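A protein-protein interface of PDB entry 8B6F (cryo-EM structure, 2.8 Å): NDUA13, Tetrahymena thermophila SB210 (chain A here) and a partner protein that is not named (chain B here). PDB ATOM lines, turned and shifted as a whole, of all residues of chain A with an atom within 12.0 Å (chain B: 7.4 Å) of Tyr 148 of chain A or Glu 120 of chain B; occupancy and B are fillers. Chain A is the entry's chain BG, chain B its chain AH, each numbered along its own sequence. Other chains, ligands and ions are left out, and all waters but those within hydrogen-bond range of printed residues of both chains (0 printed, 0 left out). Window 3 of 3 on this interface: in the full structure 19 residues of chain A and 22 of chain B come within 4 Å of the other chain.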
ATOM      1  N   ARG A 143       1.838   2.404  -7.242  1.00  0.00           N
ATOM      2  CA  ARG A 143       3.158   2.166  -6.681  1.00  0.00           C
ATOM      3  C   ARG A 143       3.656   3.465  -6.073  1.00  0.00           C
ATOM      4  O   ARG A 143       3.120   4.543  -6.340  1.00  0.00           O
ATOM      5  CB  ARG A 143       4.142   1.662  -7.742  1.00  0.00           C
ATOM      6  CG  ARG A 143       4.443   2.683  -8.831  1.00  0.00           C
ATOM      7  CD  ARG A 143       5.472   2.163  -9.808  1.00  0.00           C
ATOM      8  NE  ARG A 143       6.750   1.887  -9.163  1.00  0.00           N
ATOM      9  CZ  ARG A 143       7.723   2.775  -9.009  1.00  0.00           C
ATOM     10  NH1 ARG A 143       7.598   4.021  -9.434  1.00  0.00           N
ATOM     11  NH2 ARG A 143       8.850   2.403  -8.411  1.00  0.00           N
ATOM     12  N   TYR A 144       4.695   3.354  -5.252  1.00  0.00           N
ATOM     13  CA  TYR A 144       5.293   4.492  -4.572  1.00  0.00           C
ATOM     14  C   TYR A 144       6.663   4.778  -5.170  1.00  0.00           C
ATOM     15  O   TYR A 144       7.456   3.856  -5.384  1.00  0.00           O
ATOM     16  CB  TYR A 144       5.410   4.230  -3.070  1.00  0.00           C
ATOM     17  CG  TYR A 144       4.081   3.953  -2.411  1.00  0.00           C
ATOM     18  CD1 TYR A 144       3.514   2.688  -2.455  1.00  0.00           C
ATOM     19  CD2 TYR A 144       3.390   4.960  -1.754  1.00  0.00           C
ATOM     20  CE1 TYR A 144       2.299   2.430  -1.857  1.00  0.00           C
ATOM     21  CE2 TYR A 144       2.175   4.712  -1.154  1.00  0.00           C
ATOM     22  CZ  TYR A 144       1.635   3.445  -1.209  1.00  0.00           C
ATOM     23  OH  TYR A 144       0.422   3.194  -0.613  1.00  0.00           O
ATOM     24  N   ALA A 145       6.932   6.050  -5.442  1.00  0.00           N
ATOM     25  CA  ALA A 145       8.209   6.436  -6.023  1.00  0.00           C
ATOM     26  C   ALA A 145       9.345   6.162  -5.047  1.00  0.00           C
ATOM     27  O   ALA A 145       9.223   6.400  -3.843  1.00  0.00           O
ATOM     28  CB  ALA A 145       8.195   7.915  -6.403  1.00  0.00           C
ATOM     29  N   TYR A 146      10.455   5.651  -5.575  1.00  0.00           N
ATOM     30  CA  TYR A 146      11.646   5.376  -4.783  1.00  0.00           C
ATOM     31  C   TYR A 146      12.845   6.198  -5.227  1.00  0.00           C
ATOM     32  O   TYR A 146      13.473   6.867  -4.399  1.00  0.00           O
ATOM     33  CB  TYR A 146      11.985   3.881  -4.850  1.00  0.00           C
ATOM     34  CG  TYR A 146      13.378   3.550  -4.371  1.00  0.00           C
ATOM     35  CD1 TYR A 146      13.686   3.542  -3.019  1.00  0.00           C
ATOM     36  CD2 TYR A 146      14.382   3.232  -5.272  1.00  0.00           C
ATOM     37  CE1 TYR A 146      14.958   3.237  -2.581  1.00  0.00           C
ATOM     38  CE2 TYR A 146      15.655   2.925  -4.843  1.00  0.00           C
ATOM     39  CZ  TYR A 146      15.937   2.928  -3.497  1.00  0.00           C
ATOM     40  OH  TYR A 146      17.207   2.622  -3.067  1.00  0.00           O
ATOM     41  N   MET A 147      13.173   6.176  -6.515  1.00  0.00           N
ATOM     42  CA  MET A 147      14.377   6.835  -6.996  1.00  0.00           C
ATOM     43  C   MET A 147      14.287   8.344  -6.814  1.00  0.00           C
ATOM     44  O   MET A 147      13.203   8.933  -6.812  1.00  0.00           O
ATOM     45  CB  MET A 147      14.608   6.507  -8.471  1.00  0.00           C
ATOM     46  CG  MET A 147      15.379   5.221  -8.726  1.00  0.00           C
ATOM     47  SD  MET A 147      17.157   5.451  -8.546  1.00  0.00           S
ATOM     48  CE  MET A 147      17.427   4.783  -6.910  1.00  0.00           C
ATOM     49  N   TYR A 148      15.453   8.970  -6.664  1.00  0.00           N
ATOM     50  CA  TYR A 148      15.565  10.423  -6.553  1.00  0.00           C
ATOM     51  C   TYR A 148      14.725  10.955  -5.396  1.00  0.00           C
ATOM     52  O   TYR A 148      13.979  11.925  -5.529  1.00  0.00           O
ATOM     53  CB  TYR A 148      15.177  11.099  -7.869  1.00  0.00           C
ATOM     54  CG  TYR A 148      16.037  10.668  -9.030  1.00  0.00           C
ATOM     55  CD1 TYR A 148      17.320  11.172  -9.192  1.00  0.00           C
ATOM     56  CD2 TYR A 148      15.568   9.754  -9.962  1.00  0.00           C
ATOM     57  CE1 TYR A 148      18.112  10.778 -10.249  1.00  0.00           C
ATOM     58  CE2 TYR A 148      16.352   9.354 -11.023  1.00  0.00           C
ATOM     59  CZ  TYR A 148      17.624   9.870 -11.161  1.00  0.00           C
ATOM     60  OH  TYR A 148      18.410   9.475 -12.218  1.00  0.00           O
ATOM     61  N   ASN A 149      14.860  10.307  -4.241  1.00  0.00           N
ATOM     62  CA  ASN A 149      14.163  10.727  -3.031  1.00  0.00           C
ATOM     63  C   ASN A 149      12.654  10.766  -3.259  1.00  0.00           C
ATOM     64  O   ASN A 149      11.969  11.709  -2.859  1.00  0.00           O
ATOM     65  CB  ASN A 149      14.679  12.086  -2.556  1.00  0.00           C
ATOM     66  CG  ASN A 149      14.340  12.366  -1.110  1.00  0.00           C
ATOM     67  OD1 ASN A 149      13.317  11.916  -0.601  1.00  0.00           O
ATOM     68  ND2 ASN A 149      15.203  13.117  -0.437  1.00  0.00           N
ATOM     69  N   SER A 150      12.133   9.731  -3.918  1.00  0.00           N
ATOM     70  CA  SER A 150      10.713   9.629  -4.242  1.00  0.00           C
ATOM     71  C   SER A 150      10.272  10.814  -5.103  1.00  0.00           C
ATOM     72  O   SER A 150       9.369  11.575  -4.755  1.00  0.00           O
ATOM     73  CB  SER A 150       9.868   9.530  -2.968  1.00  0.00           C
ATOM     74  OG  SER A 150      10.122   8.315  -2.284  1.00  0.00           O
ATOM     75  N   SER A 151      10.941  10.956  -6.243  1.00  0.00           N
ATOM     76  CA  SER A 151      10.628  11.994  -7.211  1.00  0.00           C
ATOM     77  C   SER A 151      10.773  11.412  -8.610  1.00  0.00           C
ATOM     78  O   SER A 151      11.166  10.256  -8.786  1.00  0.00           O
ATOM     79  CB  SER A 151      11.528  13.217  -7.023  1.00  0.00           C
ATOM     80  OG  SER A 151      11.440  13.719  -5.701  1.00  0.00           O
ATOM     81  N   ASN A 152      10.447  12.223  -9.613  1.00  0.00           N
ATOM     82  CA  ASN A 152      10.553  11.833 -11.014  1.00  0.00           C
ATOM     83  C   ASN A 152      11.524  12.771 -11.714  1.00  0.00           C
ATOM     84  O   ASN A 152      11.272  13.977 -11.802  1.00  0.00           O
ATOM     85  CB  ASN A 152       9.186  11.867 -11.699  1.00  0.00           C
ATOM     86  CG  ASN A 152       8.256  10.791 -11.185  1.00  0.00           C
ATOM     87  OD1 ASN A 152       8.261   9.665 -11.678  1.00  0.00           O
ATOM     88  ND2 ASN A 152       7.451  11.134 -10.187  1.00  0.00           N
ATOM     89  N   LYS A 153      12.633  12.217 -12.207  1.00  0.00           N
ATOM     90  CA  LYS A 153      13.613  13.030 -12.917  1.00  0.00           C
ATOM     91  C   LYS A 153      13.082  13.469 -14.275  1.00  0.00           C
ATOM     92  O   LYS A 153      13.194  14.643 -14.646  1.00  0.00           O
ATOM     93  CB  LYS A 153      14.919  12.249 -13.080  1.00  0.00           C
ATOM     94  CG  LYS A 153      16.002  13.008 -13.838  1.00  0.00           C
ATOM     95  CD  LYS A 153      17.282  12.196 -13.968  1.00  0.00           C
ATOM     96  CE  LYS A 153      17.096  10.995 -14.882  1.00  0.00           C
ATOM     97  NZ  LYS A 153      18.373  10.257 -15.096  1.00  0.00           N
ATOM     98  N   ASN A 154      12.498  12.544 -15.028  1.00  0.00           N
ATOM     99  CA  ASN A 154      12.056  12.786 -16.398  1.00  0.00           C
ATOM    100  C   ASN A 154      10.531  12.822 -16.419  1.00  0.00           C
ATOM    101  O   ASN A 154       9.875  11.788 -16.555  1.00  0.00           O
ATOM    102  CB  ASN A 154      12.593  11.713 -17.340  1.00  0.00           C
ATOM    103  CG  ASN A 154      14.104  11.717 -17.429  1.00  0.00           C
ATOM    104  OD1 ASN A 154      14.759  10.733 -17.091  1.00  0.00           O
ATOM    105  ND2 ASN A 154      14.667  12.828 -17.894  1.00  0.00           N
ATOM    106  N   VAL A 155       9.967  14.017 -16.278  1.00  0.00           N
ATOM    107  CA  VAL A 155       8.516  14.204 -16.442  1.00  0.00           C
ATOM    108  C   VAL A 155       8.304  14.523 -17.916  1.00  0.00           C
ATOM    109  O   VAL A 155       8.116  15.670 -18.327  1.00  0.00           O
ATOM    110  CB  VAL A 155       7.967  15.293 -15.516  1.00  0.00           C
ATOM    111  CG1 VAL A 155       6.457  15.358 -15.622  1.00  0.00           C
ATOM    112  CG2 VAL A 155       8.402  15.046 -14.079  1.00  0.00           C
ATOM    113  N   LYS A 156       8.283  13.471 -18.728  1.00  0.00           N
ATOM    114  CA  LYS A 156       8.234  13.595 -20.179  1.00  0.00           C
ATOM    115  C   LYS A 156       7.924  12.222 -20.754  1.00  0.00           C
ATOM    116  O   LYS A 156       7.875  11.225 -20.032  1.00  0.00           O
ATOM    117  CB  LYS A 156       9.551  14.123 -20.758  1.00  0.00           C
ATOM    118  CG  LYS A 156       9.865  15.578 -20.443  1.00  0.00           C
ATOM    119  CD  LYS A 156      11.019  16.096 -21.286  1.00  0.00           C
ATOM    120  CE  LYS A 156      12.299  15.320 -21.027  1.00  0.00           C
ATOM    121  NZ  LYS A 156      12.704  15.343 -19.596  1.00  0.00           N
ATOM    122  N   VAL A 161      12.353  12.558 -23.774  1.00  0.00           N
ATOM    123  CA  VAL A 161      13.548  12.331 -22.967  1.00  0.00           C
ATOM    124  C   VAL A 161      14.756  12.101 -23.863  1.00  0.00           C
ATOM    125  O   VAL A 161      15.848  12.618 -23.600  1.00  0.00           O
ATOM    126  CB  VAL A 161      13.317  11.144 -22.010  1.00  0.00           C
ATOM    127  CG1 VAL A 161      14.630  10.651 -21.416  1.00  0.00           C
ATOM    128  CG2 VAL A 161      12.359  11.541 -20.902  1.00  0.00           C
ATOM    129  N   ARG A 165      17.804  16.016 -25.116  1.00  0.00           N
ATOM    130  CA  ARG A 165      19.224  16.106 -24.804  1.00  0.00           C
ATOM    131  C   ARG A 165      20.055  16.584 -25.988  1.00  0.00           C
ATOM    132  O   ARG A 165      21.220  16.946 -25.798  1.00  0.00           O
ATOM    133  CB  ARG A 165      19.737  14.746 -24.322  1.00  0.00           C
ATOM    134  CG  ARG A 165      21.114  14.780 -23.664  1.00  0.00           C
ATOM    135  CD  ARG A 165      21.103  15.585 -22.372  1.00  0.00           C
ATOM    136  NE  ARG A 165      22.387  15.532 -21.684  1.00  0.00           N
ATOM    137  CZ  ARG A 165      22.672  16.203 -20.575  1.00  0.00           C
ATOM    138  NH1 ARG A 165      21.784  16.995 -19.998  1.00  0.00           N
ATOM    139  NH2 ARG A 165      23.878  16.074 -20.030  1.00  0.00           N
ATOM    140  N   ASN B 107      30.571   7.749 -19.962  1.00  0.00           N
ATOM    141  CA  ASN B 107      30.806   7.905 -18.529  1.00  0.00           C
ATOM    142  C   ASN B 107      32.023   8.797 -18.285  1.00  0.00           C
ATOM    143  O   ASN B 107      33.035   8.387 -17.721  1.00  0.00           O
ATOM    144  CB  ASN B 107      30.977   6.536 -17.879  1.00  0.00           C
ATOM    145  CG  ASN B 107      31.046   6.612 -16.371  1.00  0.00           C
ATOM    146  OD1 ASN B 107      30.486   7.519 -15.759  1.00  0.00           O
ATOM    147  ND2 ASN B 107      31.732   5.654 -15.763  1.00  0.00           N
ATOM    148  N   PHE B 117      25.347  12.645 -20.887  1.00  0.00           N
ATOM    149  CA  PHE B 117      24.141  12.162 -20.236  1.00  0.00           C
ATOM    150  C   PHE B 117      24.203  12.488 -18.752  1.00  0.00           C
ATOM    151  O   PHE B 117      25.284  12.629 -18.174  1.00  0.00           O
ATOM    152  CB  PHE B 117      23.964  10.653 -20.427  1.00  0.00           C
ATOM    153  CG  PHE B 117      23.858  10.225 -21.859  1.00  0.00           C
ATOM    154  CD1 PHE B 117      23.277  11.047 -22.810  1.00  0.00           C
ATOM    155  CD2 PHE B 117      24.341   8.992 -22.253  1.00  0.00           C
ATOM    156  CE1 PHE B 117      23.184  10.645 -24.126  1.00  0.00           C
ATOM    157  CE2 PHE B 117      24.251   8.584 -23.564  1.00  0.00           C
ATOM    158  CZ  PHE B 117      23.672   9.411 -24.504  1.00  0.00           C
ATOM    159  N   ASP B 118      23.028  12.609 -18.137  1.00  0.00           N
ATOM    160  CA  ASP B 118      22.924  12.926 -16.712  1.00  0.00           C
ATOM    161  C   ASP B 118      22.986  11.638 -15.889  1.00  0.00           C
ATOM    162  O   ASP B 118      22.016  11.197 -15.271  1.00  0.00           O
ATOM    163  CB  ASP B 118      21.648  13.712 -16.435  1.00  0.00           C
ATOM    164  CG  ASP B 118      20.405  12.999 -16.925  1.00  0.00           C
ATOM    165  OD1 ASP B 118      20.534  11.882 -17.468  1.00  0.00           O
ATOM    166  OD2 ASP B 118      19.297  13.554 -16.771  1.00  0.00           O
ATOM    167  N   LEU B 119      24.172  11.037 -15.890  1.00  0.00           N
ATOM    168  CA  LEU B 119      24.423   9.811 -15.147  1.00  0.00           C
ATOM    169  C   LEU B 119      24.880  10.133 -13.733  1.00  0.00           C
ATOM    170  O   LEU B 119      25.681  11.045 -13.516  1.00  0.00           O
ATOM    171  CB  LEU B 119      25.481   8.958 -15.847  1.00  0.00           C
ATOM    172  CG  LEU B 119      24.977   7.964 -16.893  1.00  0.00           C
ATOM    173  CD1 LEU B 119      23.974   8.625 -17.804  1.00  0.00           C
ATOM    174  CD2 LEU B 119      26.140   7.417 -17.697  1.00  0.00           C
ATOM    175  N   GLU B 120      24.360   9.372 -12.773  1.00  0.00           N
ATOM    176  CA  GLU B 120      24.736   9.497 -11.373  1.00  0.00           C
ATOM    177  C   GLU B 120      25.717   8.423 -10.933  1.00  0.00           C
ATOM    178  O   GLU B 120      26.673   8.721 -10.212  1.00  0.00           O
ATOM    179  CB  GLU B 120      23.488   9.431 -10.486  1.00  0.00           C
ATOM    180  CG  GLU B 120      23.771   9.617  -9.002  1.00  0.00           C
ATOM    181  CD  GLU B 120      22.516   9.522  -8.157  1.00  0.00           C
ATOM    182  OE1 GLU B 120      21.447   9.202  -8.715  1.00  0.00           O
ATOM    183  OE2 GLU B 120      22.598   9.765  -6.935  1.00  0.00           O
ATOM    184  N   TYR B 121      25.505   7.180 -11.356  1.00  0.00           N
ATOM    185  CA  TYR B 121      26.337   6.061 -10.921  1.00  0.00           C
ATOM    186  C   TYR B 121      27.507   5.862 -11.887  1.00  0.00           C
ATOM    187  O   TYR B 121      27.635   4.847 -12.570  1.00  0.00           O
ATOM    188  CB  TYR B 121      25.492   4.798 -10.801  1.00  0.00           C
ATOM    189  CG  TYR B 121      24.208   4.998 -10.027  1.00  0.00           C
ATOM    190  CD1 TYR B 121      24.128   5.933  -9.003  1.00  0.00           C
ATOM    191  CD2 TYR B 121      23.074   4.254 -10.324  1.00  0.00           C
ATOM    192  CE1 TYR B 121      22.958   6.122  -8.296  1.00  0.00           C
ATOM    193  CE2 TYR B 121      21.897   4.437  -9.622  1.00  0.00           C
ATOM    194  CZ  TYR B 121      21.847   5.371  -8.610  1.00  0.00           C
ATOM    195  OH  TYR B 121      20.683   5.559  -7.905  1.00  0.00           O
ATOM    196  N   ASN B 122      28.377   6.873 -11.930  1.00  0.00           N
ATOM    197  CA  ASN B 122      29.518   6.823 -12.837  1.00  0.00           C
ATOM    198  C   ASN B 122      30.452   5.674 -12.487  1.00  0.00           C
ATOM    199  O   ASN B 122      30.956   4.980 -13.377  1.00  0.00           O
ATOM    200  CB  ASN B 122      30.274   8.150 -12.804  1.00  0.00           C
ATOM    201  CG  ASN B 122      29.462   9.295 -13.368  1.00  0.00           C
ATOM    202  OD1 ASN B 122      29.220  10.292 -12.690  1.00  0.00           O
ATOM    203  ND2 ASN B 122      29.042   9.161 -14.619  1.00  0.00           N
ATOM    204  N   LEU B 123      30.702   5.459 -11.195  1.00  0.00           N
ATOM    205  CA  LEU B 123      31.583   4.372 -10.790  1.00  0.00           C
ATOM    206  C   LEU B 123      30.970   3.018 -11.120  1.00  0.00           C
ATOM    207  O   LEU B 123      31.680   2.094 -11.533  1.00  0.00           O
ATOM    208  CB  LEU B 123      31.897   4.485  -9.300  1.00  0.00           C
ATOM    209  CG  LEU B 123      32.576   5.796  -8.888  1.00  0.00           C
ATOM    210  CD1 LEU B 123      32.823   5.819  -7.401  1.00  0.00           C
ATOM    211  CD2 LEU B 123      33.885   6.006  -9.632  1.00  0.00           C
ATOM    212  N   VAL B 124      29.658   2.875 -10.937  1.00  0.00           N
ATOM    213  CA  VAL B 124      28.993   1.631 -11.312  1.00  0.00           C
ATOM    214  C   VAL B 124      29.119   1.401 -12.811  1.00  0.00           C
ATOM    215  O   VAL B 124      29.404   0.285 -13.261  1.00  0.00           O
ATOM    216  CB  VAL B 124      27.520   1.657 -10.862  1.00  0.00           C
ATOM    217  CG1 VAL B 124      26.770   0.439 -11.388  1.00  0.00           C
ATOM    218  CG2 VAL B 124      27.433   1.724  -9.349  1.00  0.00           C
ATOM    219  N   TYR B 125      28.909   2.450 -13.606  1.00  0.00           N
ATOM    220  CA  TYR B 125      29.067   2.325 -15.051  1.00  0.00           C
ATOM    221  C   TYR B 125      30.484   1.902 -15.410  1.00  0.00           C
ATOM    222  O   TYR B 125      30.682   1.024 -16.256  1.00  0.00           O
ATOM    223  CB  TYR B 125      28.716   3.645 -15.734  1.00  0.00           C
ATOM    224  CG  TYR B 125      27.317   3.687 -16.297  1.00  0.00           C
ATOM    225  CD1 TYR B 125      26.217   3.437 -15.489  1.00  0.00           C
ATOM    226  CD2 TYR B 125      27.095   3.993 -17.632  1.00  0.00           C
ATOM    227  CE1 TYR B 125      24.935   3.477 -15.997  1.00  0.00           C
ATOM    228  CE2 TYR B 125      25.814   4.036 -18.151  1.00  0.00           C
ATOM    229  CZ  TYR B 125      24.740   3.777 -17.328  1.00  0.00           C
ATOM    230  OH  TYR B 125      23.463   3.819 -17.836  1.00  0.00           O
ATOM    231  N   GLU B 179      30.184  10.699  -0.758  1.00  0.00           N
ATOM    232  CA  GLU B 179      28.834  10.211  -0.486  1.00  0.00           C
ATOM    233  C   GLU B 179      28.000  10.060  -1.753  1.00  0.00           C
ATOM    234  O   GLU B 179      26.768  10.082  -1.688  1.00  0.00           O
ATOM    235  CB  GLU B 179      28.098  11.123   0.504  1.00  0.00           C
ATOM    236  CG  GLU B 179      28.872  11.411   1.781  1.00  0.00           C
ATOM    237  CD  GLU B 179      28.128  12.349   2.711  1.00  0.00           C
ATOM    238  OE1 GLU B 179      26.962  12.681   2.411  1.00  0.00           O
ATOM    239  OE2 GLU B 179      28.708  12.759   3.738  1.00  0.00           O
ATOM    240  N   SER B 180      28.642   9.914  -2.909  1.00  0.00           N
ATOM    241  CA  SER B 180      27.923   9.721  -4.160  1.00  0.00           C
ATOM    242  C   SER B 180      28.846   9.053  -5.164  1.00  0.00           C
ATOM    243  O   SER B 180      30.070   9.069  -5.018  1.00  0.00           O
ATOM    244  CB  SER B 180      27.428  11.041  -4.738  1.00  0.00           C
ATOM    245  OG  SER B 180      28.544  11.824  -5.100  1.00  0.00           O
ATOM    246  N   PHE B 181      28.239   8.462  -6.189  1.00  0.00           N
ATOM    247  CA  PHE B 181      28.984   7.860  -7.284  1.00  0.00           C
ATOM    248  C   PHE B 181      29.281   8.842  -8.408  1.00  0.00           C
ATOM    249  O   PHE B 181      30.024   8.493  -9.332  1.00  0.00           O
ATOM    250  CB  PHE B 181      28.208   6.670  -7.858  1.00  0.00           C
ATOM    251  CG  PHE B 181      28.135   5.486  -6.937  1.00  0.00           C
ATOM    252  CD1 PHE B 181      29.239   5.084  -6.205  1.00  0.00           C
ATOM    253  CD2 PHE B 181      26.955   4.775  -6.807  1.00  0.00           C
ATOM    254  CE1 PHE B 181      29.170   3.996  -5.361  1.00  0.00           C
ATOM    255  CE2 PHE B 181      26.878   3.686  -5.965  1.00  0.00           C
ATOM    256  CZ  PHE B 181      27.986   3.295  -5.240  1.00  0.00           C
ATOM    257  N   CYS B 182      28.728  10.050  -8.357  1.00  0.00           N
ATOM    258  CA  CYS B 182      28.957  11.034  -9.403  1.00  0.00           C
ATOM    259  C   CYS B 182      30.324  11.685  -9.238  1.00  0.00           C
ATOM    260  O   CYS B 182      30.762  11.974  -8.122  1.00  0.00           O
ATOM    261  CB  CYS B 182      27.866  12.105  -9.375  1.00  0.00           C
ATOM    262  SG  CYS B 182      27.972  13.309 -10.716  1.00  0.00           S
ATOM    263  N   PHE B 183      30.996  11.918 -10.366  1.00  0.00           N
ATOM    264  CA  PHE B 183      32.323  12.520 -10.327  1.00  0.00           C
ATOM    265  C   PHE B 183      32.289  13.964  -9.842  1.00  0.00           C
ATOM    266  O   PHE B 183      33.268  14.441  -9.258  1.00  0.00           O
ATOM    267  CB  PHE B 183      32.967  12.454 -11.712  1.00  0.00           C
ATOM    268  CG  PHE B 183      33.235  11.060 -12.201  1.00  0.00           C
ATOM    269  CD1 PHE B 183      33.591  10.052 -11.320  1.00  0.00           C
ATOM    270  CD2 PHE B 183      33.146  10.765 -13.550  1.00  0.00           C
ATOM    271  CE1 PHE B 183      33.842   8.774 -11.776  1.00  0.00           C
ATOM    272  CE2 PHE B 183      33.397   9.489 -14.011  1.00  0.00           C
ATOM    273  CZ  PHE B 183      33.748   8.493 -13.123  1.00  0.00           C
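Among the printed residues, pairs that only touch across the chains: Tyr 148 of chain A with Glu 120 of chain B (3.99 Å) and Arg 165 of chain A with Phe 117 of chain B (3.8 Å).
Of the 16 printed residues of chain A, 4 touch a printed residue of chain B. Hydrophobic or aromatic side chains of chain A that line the printed part of chain B: Met 147 and Tyr 148. Among the printed residues, 4 pairs touch across the chains.
The side-chain carboxylate (OD1) of Asp 118 of chain B lies within salt-bridge range of the side-chain amino group (NZ) of Lys 153 of chain A (3.6 Å). OH of Tyr 121 of chain B sits close to SD of Met 147 of chain A (3.6 Å).
Printed residues of chain B within 4 Å of Tyr 148 of chain A: Glu 120 (3.99 Å). Printed residues of chain A within 4 Å of Glu 120 of chain B: Tyr 148. Of the printed residues of chain A, Asp 118 of chain B touches Lys 153. No residue of chain A comes within 4 Å of Leu 119 of chain B. Of chain A, only Met 147 comes within 4 Å of Tyr 121 of chain B. No residue of chain A comes within 4 Å of Asn 122 of chain B. No residue of chain A comes within 4 Å of Ser 180 of chain B. No residue of chain A comes within 4 Å of Phe 181 of chain B. No residue of chain A comes within 4 Å of Cys 182 of chain B. Of the printed residues of chain B, Lys 153 of chain A touches Asp 118. Of the printed residues of chain B, Met 147 of chain A touches Tyr 121. Leu 123 of chain B touches none of the printed residues of chain A. The nearest printed residue of chain A that does not touch Glu 120 of chain B is Met 147 of chain A (5.7 Å). The nearest printed residue of chain B that does not touch Arg 165 of chain A is Asp 118 of chain B (4.04 Å).
O of Glu 120 of chain B sits at hydrogen-bond distance from N of Cys 182 of chain B (3.1 Å). O of Tyr 148 of chain A sits at hydrogen-bond distance from OG of Ser 151 of chain A (3.1 Å). The side-chain hydroxyl (OH) of Tyr 148 of chain A is in hydrogen-bond range of the side-chain amino group (NZ) of Lys 153 of chain A (3.0 Å).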
